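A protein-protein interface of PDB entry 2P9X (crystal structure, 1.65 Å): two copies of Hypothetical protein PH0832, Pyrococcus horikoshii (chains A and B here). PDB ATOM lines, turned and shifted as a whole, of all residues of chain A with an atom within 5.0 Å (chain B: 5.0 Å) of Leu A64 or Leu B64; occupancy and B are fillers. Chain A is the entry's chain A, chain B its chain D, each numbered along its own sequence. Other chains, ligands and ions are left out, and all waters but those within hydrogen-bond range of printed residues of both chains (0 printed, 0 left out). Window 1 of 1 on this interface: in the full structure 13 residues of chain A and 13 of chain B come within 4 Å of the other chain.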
ATOM      1  N   VAL A  19      20.552  17.944  16.771  1.00  0.00           N
ATOM      2  CA  VAL A  19      21.564  18.987  16.695  1.00  0.00           C
ATOM      3  C   VAL A  19      21.193  20.191  17.552  1.00  0.00           C
ATOM      4  O   VAL A  19      21.937  20.583  18.455  1.00  0.00           O
ATOM      5  CB  VAL A  19      21.758  19.475  15.242  1.00  0.00           C
ATOM      6  CG1 VAL A  19      22.693  20.680  15.219  1.00  0.00           C
ATOM      7  CG2 VAL A  19      22.330  18.348  14.396  1.00  0.00           C
ATOM      8  N   GLU A  59      30.652  24.570   2.902  1.00  0.00           N
ATOM      9  CA  GLU A  59      30.942  23.165   2.634  1.00  0.00           C
ATOM     10  C   GLU A  59      31.409  22.347   3.834  1.00  0.00           C
ATOM     11  O   GLU A  59      31.148  21.144   3.908  1.00  0.00           O
ATOM     12  CB  GLU A  59      31.969  23.058   1.508  1.00  0.00           C
ATOM     13  CG  GLU A  59      32.193  21.639   1.031  1.00  0.00           C
ATOM     14  CD  GLU A  59      33.168  21.574  -0.122  1.00  0.00           C
ATOM     15  OE1 GLU A  59      32.902  22.224  -1.156  1.00  0.00           O
ATOM     16  OE2 GLU A  59      34.196  20.874   0.007  1.00  0.00           O
ATOM     17  N   TYR A  60      32.100  22.986   4.768  1.00  0.00           N
ATOM     18  CA  TYR A  60      32.573  22.285   5.954  1.00  0.00           C
ATOM     19  C   TYR A  60      31.366  21.815   6.767  1.00  0.00           C
ATOM     20  O   TYR A  60      31.288  20.656   7.184  1.00  0.00           O
ATOM     21  CB  TYR A  60      33.462  23.208   6.792  1.00  0.00           C
ATOM     22  CG  TYR A  60      34.726  23.623   6.069  1.00  0.00           C
ATOM     23  CD1 TYR A  60      35.716  22.690   5.772  1.00  0.00           C
ATOM     24  CD2 TYR A  60      34.908  24.937   5.632  1.00  0.00           C
ATOM     25  CE1 TYR A  60      36.855  23.046   5.053  1.00  0.00           C
ATOM     26  CE2 TYR A  60      36.045  25.304   4.907  1.00  0.00           C
ATOM     27  CZ  TYR A  60      37.014  24.349   4.622  1.00  0.00           C
ATOM     28  OH  TYR A  60      38.131  24.688   3.893  1.00  0.00           O
ATOM     29  N   SER A  61      30.411  22.716   6.975  1.00  0.00           N
ATOM     30  CA  SER A  61      29.211  22.373   7.721  1.00  0.00           C
ATOM     31  C   SER A  61      28.365  21.347   6.974  1.00  0.00           C
ATOM     32  O   SER A  61      27.805  20.437   7.587  1.00  0.00           O
ATOM     33  CB  SER A  61      28.390  23.637   7.995  1.00  0.00           C
ATOM     34  OG  SER A  61      27.265  23.317   8.799  1.00  0.00           O
ATOM     35  N   ALA A  62      28.278  21.486   5.653  1.00  0.00           N
ATOM     36  CA  ALA A  62      27.494  20.553   4.843  1.00  0.00           C
ATOM     37  C   ALA A  62      28.093  19.160   4.954  1.00  0.00           C
ATOM     38  O   ALA A  62      27.368  18.167   5.060  1.00  0.00           O
ATOM     39  CB  ALA A  62      27.475  20.997   3.379  1.00  0.00           C
ATOM     40  N   ARG A  63      29.419  19.087   4.930  1.00  0.00           N
ATOM     41  CA  ARG A  63      30.098  17.799   5.042  1.00  0.00           C
ATOM     42  C   ARG A  63      29.809  17.152   6.393  1.00  0.00           C
ATOM     43  O   ARG A  63      29.544  15.952   6.462  1.00  0.00           O
ATOM     44  CB  ARG A  63      31.609  17.971   4.854  1.00  0.00           C
ATOM     45  CG  ARG A  63      32.054  17.856   3.400  1.00  0.00           C
ATOM     46  CD  ARG A  63      31.890  16.422   2.909  1.00  0.00           C
ATOM     47  NE  ARG A  63      32.821  15.525   3.589  1.00  0.00           N
ATOM     48  CZ  ARG A  63      32.562  14.260   3.898  1.00  0.00           C
ATOM     49  NH1 ARG A  63      31.385  13.719   3.593  1.00  0.00           N
ATOM     50  NH2 ARG A  63      33.482  13.532   4.509  1.00  0.00           N
ATOM     51  N   LEU A  64      29.863  17.950   7.459  1.00  0.00           N
ATOM     52  CA  LEU A  64      29.592  17.449   8.803  1.00  0.00           C
ATOM     53  C   LEU A  64      28.177  16.873   8.870  1.00  0.00           C
ATOM     54  O   LEU A  64      27.971  15.797   9.429  1.00  0.00           O
ATOM     55  CB  LEU A  64      29.774  18.571   9.840  1.00  0.00           C
ATOM     56  CG  LEU A  64      31.229  18.971  10.137  1.00  0.00           C
ATOM     57  CD1 LEU A  64      31.275  20.235  10.981  1.00  0.00           C
ATOM     58  CD2 LEU A  64      31.927  17.827  10.875  1.00  0.00           C
ATOM     59  N   LEU A  65      27.203  17.580   8.296  1.00  0.00           N
ATOM     60  CA  LEU A  65      25.827  17.090   8.298  1.00  0.00           C
ATOM     61  C   LEU A  65      25.742  15.778   7.516  1.00  0.00           C
ATOM     62  O   LEU A  65      25.069  14.833   7.932  1.00  0.00           O
ATOM     63  CB  LEU A  65      24.881  18.125   7.675  1.00  0.00           C
ATOM     64  CG  LEU A  65      23.418  17.678   7.580  1.00  0.00           C
ATOM     65  CD1 LEU A  65      22.858  17.409   8.975  1.00  0.00           C
ATOM     66  CD2 LEU A  65      22.606  18.754   6.872  1.00  0.00           C
ATOM     67  N   GLU A  66      26.438  15.719   6.385  1.00  0.00           N
ATOM     68  CA  GLU A  66      26.441  14.513   5.563  1.00  0.00           C
ATOM     69  C   GLU A  66      26.957  13.337   6.393  1.00  0.00           C
ATOM     70  O   GLU A  66      26.345  12.271   6.424  1.00  0.00           O
ATOM     71  CB  GLU A  66      27.329  14.716   4.332  1.00  0.00           C
ATOM     72  CG  GLU A  66      27.259  13.590   3.313  1.00  0.00           C
ATOM     73  CD  GLU A  66      28.112  13.856   2.079  1.00  0.00           C
ATOM     74  OE1 GLU A  66      29.242  14.376   2.218  1.00  0.00           O
ATOM     75  OE2 GLU A  66      27.659  13.532   0.963  1.00  0.00           O
ATOM     76  N   MET A  67      28.079  13.542   7.076  1.00  0.00           N
ATOM     77  CA  MET A  67      28.663  12.489   7.902  1.00  0.00           C
ATOM     78  C   MET A  67      27.692  12.035   8.985  1.00  0.00           C
ATOM     79  O   MET A  67      27.551  10.836   9.243  1.00  0.00           O
ATOM     80  CB  MET A  67      29.961  12.988   8.532  1.00  0.00           C
ATOM     81  CG  MET A  67      31.091  13.095   7.524  1.00  0.00           C
ATOM     82  SD  MET A  67      32.484  14.064   8.119  1.00  0.00           S
ATOM     83  CE  MET A  67      33.168  12.943   9.340  1.00  0.00           C
ATOM     84  N   VAL A  68      27.025  12.993   9.619  1.00  0.00           N
ATOM     85  CA  VAL A  68      26.066  12.680  10.663  1.00  0.00           C
ATOM     86  C   VAL A  68      24.873  11.903  10.101  1.00  0.00           C
ATOM     87  O   VAL A  68      24.428  10.928  10.704  1.00  0.00           O
ATOM     88  CB  VAL A  68      25.584  13.967  11.363  1.00  0.00           C
ATOM     89  CG1 VAL A  68      24.397  13.665  12.252  1.00  0.00           C
ATOM     90  CG2 VAL A  68      26.723  14.553  12.198  1.00  0.00           C
ATOM     91  N   VAL B  19      36.552  15.504   7.145  1.00  0.00           N
ATOM     92  CA  VAL B  19      35.548  16.454   6.688  1.00  0.00           C
ATOM     93  C   VAL B  19      36.015  17.066   5.374  1.00  0.00           C
ATOM     94  O   VAL B  19      35.336  16.977   4.355  1.00  0.00           O
ATOM     95  CB  VAL B  19      35.340  17.579   7.724  1.00  0.00           C
ATOM     96  CG1 VAL B  19      34.422  18.660   7.159  1.00  0.00           C
ATOM     97  CG2 VAL B  19      34.754  16.996   9.000  1.00  0.00           C
ATOM     98  N   GLU B  59      26.488  27.967  15.861  1.00  0.00           N
ATOM     99  CA  GLU B  59      26.137  26.896  16.793  1.00  0.00           C
ATOM    100  C   GLU B  59      25.681  25.592  16.146  1.00  0.00           C
ATOM    101  O   GLU B  59      25.943  24.510  16.678  1.00  0.00           O
ATOM    102  CB  GLU B  59      25.059  27.401  17.754  1.00  0.00           C
ATOM    103  CG  GLU B  59      24.589  26.396  18.788  1.00  0.00           C
ATOM    104  CD  GLU B  59      23.555  26.990  19.726  1.00  0.00           C
ATOM    105  OE1 GLU B  59      23.933  27.836  20.571  1.00  0.00           O
ATOM    106  OE2 GLU B  59      22.367  26.618  19.608  1.00  0.00           O
ATOM    107  N   TYR B  60      24.994  25.681  15.012  1.00  0.00           N
ATOM    108  CA  TYR B  60      24.520  24.471  14.347  1.00  0.00           C
ATOM    109  C   TYR B  60      25.716  23.676  13.852  1.00  0.00           C
ATOM    110  O   TYR B  60      25.806  22.471  14.069  1.00  0.00           O
ATOM    111  CB  TYR B  60      23.591  24.825  13.176  1.00  0.00           C
ATOM    112  CG  TYR B  60      22.355  25.576  13.618  1.00  0.00           C
ATOM    113  CD1 TYR B  60      21.402  24.962  14.431  1.00  0.00           C
ATOM    114  CD2 TYR B  60      22.156  26.906  13.255  1.00  0.00           C
ATOM    115  CE1 TYR B  60      20.278  25.659  14.876  1.00  0.00           C
ATOM    116  CE2 TYR B  60      21.031  27.617  13.699  1.00  0.00           C
ATOM    117  CZ  TYR B  60      20.102  26.985  14.507  1.00  0.00           C
ATOM    118  OH  TYR B  60      19.003  27.676  14.956  1.00  0.00           O
ATOM    119  N   SER B  61      26.644  24.357  13.195  1.00  0.00           N
ATOM    120  CA  SER B  61      27.838  23.693  12.689  1.00  0.00           C
ATOM    121  C   SER B  61      28.693  23.180  13.845  1.00  0.00           C
ATOM    122  O   SER B  61      29.265  22.098  13.757  1.00  0.00           O
ATOM    123  CB  SER B  61      28.651  24.659  11.830  1.00  0.00           C
ATOM    124  OG  SER B  61      27.836  25.223  10.814  1.00  0.00           O
ATOM    125  N   ALA B  62      28.764  23.950  14.929  1.00  0.00           N
ATOM    126  CA  ALA B  62      29.553  23.557  16.093  1.00  0.00           C
ATOM    127  C   ALA B  62      29.003  22.273  16.696  1.00  0.00           C
ATOM    128  O   ALA B  62      29.764  21.380  17.085  1.00  0.00           O
ATOM    129  CB  ALA B  62      29.545  24.666  17.138  1.00  0.00           C
ATOM    130  N   ARG B  63      27.679  22.188  16.780  1.00  0.00           N
ATOM    131  CA  ARG B  63      27.038  21.003  17.319  1.00  0.00           C
ATOM    132  C   ARG B  63      27.319  19.802  16.423  1.00  0.00           C
ATOM    133  O   ARG B  63      27.557  18.699  16.914  1.00  0.00           O
ATOM    134  CB  ARG B  63      25.536  21.244  17.450  1.00  0.00           C
ATOM    135  CG  ARG B  63      25.164  21.863  18.793  1.00  0.00           C
ATOM    136  CD  ARG B  63      25.325  20.822  19.899  1.00  0.00           C
ATOM    137  NE  ARG B  63      24.334  19.759  19.761  1.00  0.00           N
ATOM    138  CZ  ARG B  63      24.538  18.485  20.078  1.00  0.00           C
ATOM    139  NH1 ARG B  63      25.711  18.088  20.561  1.00  0.00           N
ATOM    140  NH2 ARG B  63      23.566  17.601  19.903  1.00  0.00           N
ATOM    141  N   LEU B  64      27.288  20.007  15.109  1.00  0.00           N
ATOM    142  CA  LEU B  64      27.567  18.908  14.195  1.00  0.00           C
ATOM    143  C   LEU B  64      28.990  18.410  14.418  1.00  0.00           C
ATOM    144  O   LEU B  64      29.233  17.204  14.432  1.00  0.00           O
ATOM    145  CB  LEU B  64      27.375  19.356  12.741  1.00  0.00           C
ATOM    146  CG  LEU B  64      25.909  19.498  12.317  1.00  0.00           C
ATOM    147  CD1 LEU B  64      25.832  20.235  10.995  1.00  0.00           C
ATOM    148  CD2 LEU B  64      25.262  18.118  12.219  1.00  0.00           C
ATOM    149  N   LEU B  65      29.930  19.332  14.610  1.00  0.00           N
ATOM    150  CA  LEU B  65      31.316  18.921  14.834  1.00  0.00           C
ATOM    151  C   LEU B  65      31.422  18.140  16.143  1.00  0.00           C
ATOM    152  O   LEU B  65      32.120  17.131  16.218  1.00  0.00           O
ATOM    153  CB  LEU B  65      32.249  20.139  14.880  1.00  0.00           C
ATOM    154  CG  LEU B  65      33.733  19.773  15.025  1.00  0.00           C
ATOM    155  CD1 LEU B  65      34.188  18.979  13.800  1.00  0.00           C
ATOM    156  CD2 LEU B  65      34.573  21.033  15.177  1.00  0.00           C
ATOM    157  N   GLU B  66      30.725  18.612  17.172  1.00  0.00           N
ATOM    158  CA  GLU B  66      30.743  17.938  18.467  1.00  0.00           C
ATOM    159  C   GLU B  66      30.255  16.503  18.310  1.00  0.00           C
ATOM    160  O   GLU B  66      30.858  15.558  18.832  1.00  0.00           O
ATOM    161  CB  GLU B  66      29.845  18.679  19.459  1.00  0.00           C
ATOM    162  CG  GLU B  66      29.836  18.083  20.861  1.00  0.00           C
ATOM    163  CD  GLU B  66      29.086  18.959  21.851  1.00  0.00           C
ATOM    164  OE1 GLU B  66      28.132  19.653  21.435  1.00  0.00           O
ATOM    165  OE2 GLU B  66      29.443  18.957  23.050  1.00  0.00           O
ATOM    166  N   MET B  67      29.162  16.341  17.576  1.00  0.00           N
ATOM    167  CA  MET B  67      28.585  15.025  17.346  1.00  0.00           C
ATOM    168  C   MET B  67      29.555  14.114  16.605  1.00  0.00           C
ATOM    169  O   MET B  67      29.678  12.937  16.932  1.00  0.00           O
ATOM    170  CB  MET B  67      27.280  15.168  16.561  1.00  0.00           C
ATOM    171  CG  MET B  67      26.114  15.619  17.434  1.00  0.00           C
ATOM    172  SD  MET B  67      24.682  16.186  16.489  1.00  0.00           S
ATOM    173  CE  MET B  67      23.922  14.625  16.074  1.00  0.00           C
ATOM    174  N   VAL B  68      30.239  14.659  15.602  1.00  0.00           N
ATOM    175  CA  VAL B  68      31.193  13.869  14.834  1.00  0.00           C
ATOM    176  C   VAL B  68      32.379  13.469  15.703  1.00  0.00           C
ATOM    177  O   VAL B  68      32.806  12.315  15.679  1.00  0.00           O
ATOM    178  CB  VAL B  68      31.702  14.644  13.603  1.00  0.00           C
ATOM    179  CG1 VAL B  68      32.873  13.894  12.965  1.00  0.00           C
ATOM    180  CG2 VAL B  68      30.578  14.802  12.599  1.00  0.00           C
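The side-chain carboxylate (OE1) of Glu A66 is in salt-bridge range of the guanidinium group (NH1) of Arg A63 (2.6 Å). OE1 of Glu B66 is in salt-bridge range of NH1 of Arg B63, at 3.0 Å. The guanidinium group (NH2) of Arg A63 lies within hydrogen-bond range of the side-chain sulfur (SD) of Met A67.
Of chain B, only Val B19 (3.5 Å), Ser B61 (3.9 Å), Leu B64 (3.8 Å), Leu B65 (3.9 Å) and Val B68 (3.7 Å) come within 4 Å of Leu A64. Of the printed residues of chain A, Leu B64 touches Val A19 (3.7 Å), Ser A61 (3.9 Å), Leu A64 (3.8 Å) and Val A68 (3.9 Å). Of the printed residues of chain B, Met A67 touches Val B19 (3.8 Å) and Val B68 (3.8 Å). Printed residues of chain B within 4 Å of Ser A61: Ser B61 and Leu B64. Printed residues of chain A within 4 Å of Val B68: Leu A64 (3.7 Å), Met A67 (3.8 Å) and Val A68 (3.9 Å). Of the printed residues of chain B, Tyr A60 touches Val B19 (3.7 Å). Printed residues of chain B within 4 Å of Arg A63: Val B19 (3.0 Å). Ala B62 touches none of the printed residues of chain A. The nearest printed residue of chain B that does not touch Leu A64 is Ala B62 (6.0 Å).
Hydrophobic or aromatic side chains of chain A within 4 Å of the printed part of chain B: Val A19, Leu A64, Met A67 and Val A68. Along chain A the printed residues that touch a printed residue of chain B span positions 19 to 68. Among the printed residues, 18 pairs touch across the chains.
Val A19 touches Leu B64, and with the chains exchanged Leu A64 touches Val B19. Val A19 touches Met B67, and with the chains exchanged Met A67 touches Val B19. Ser B61 touches its own counterpart, Ser A61. Met A67 touches Val B68, and with the chains exchanged Val A68 touches Met B67. 11 positions are printed for both chains.
OG of Ser A61 is in hydrogen-bond range of OG of Ser B61, at 2.8 Å. The guanidinium group (NE) of Arg A63 lies within hydrogen-bond range of the backbone carbonyl oxygen (O) of Val B19 (3.0 Å). The backbone carbonyl oxygen of Val A19 lies within hydrogen-bond range of the guanidinium group of Arg B63.
Among the printed residues, pairs that only touch across the chains: Val A19 with Tyr B60, Val A19 with Leu B64, Val A19 with Met B67, Tyr A60 with Val B19, Ser A61 with Leu B64, Leu A64 with Val B19, Leu A64 with Ser B61, Leu A64 with Leu B64, Leu A64 with Leu B65, Leu A64 with Val B68, Met A67 with Val B19, Met A67 with Val B68, Val A68 with Leu B64, Val A68 with Met B67 and Val A68 with Val B68.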
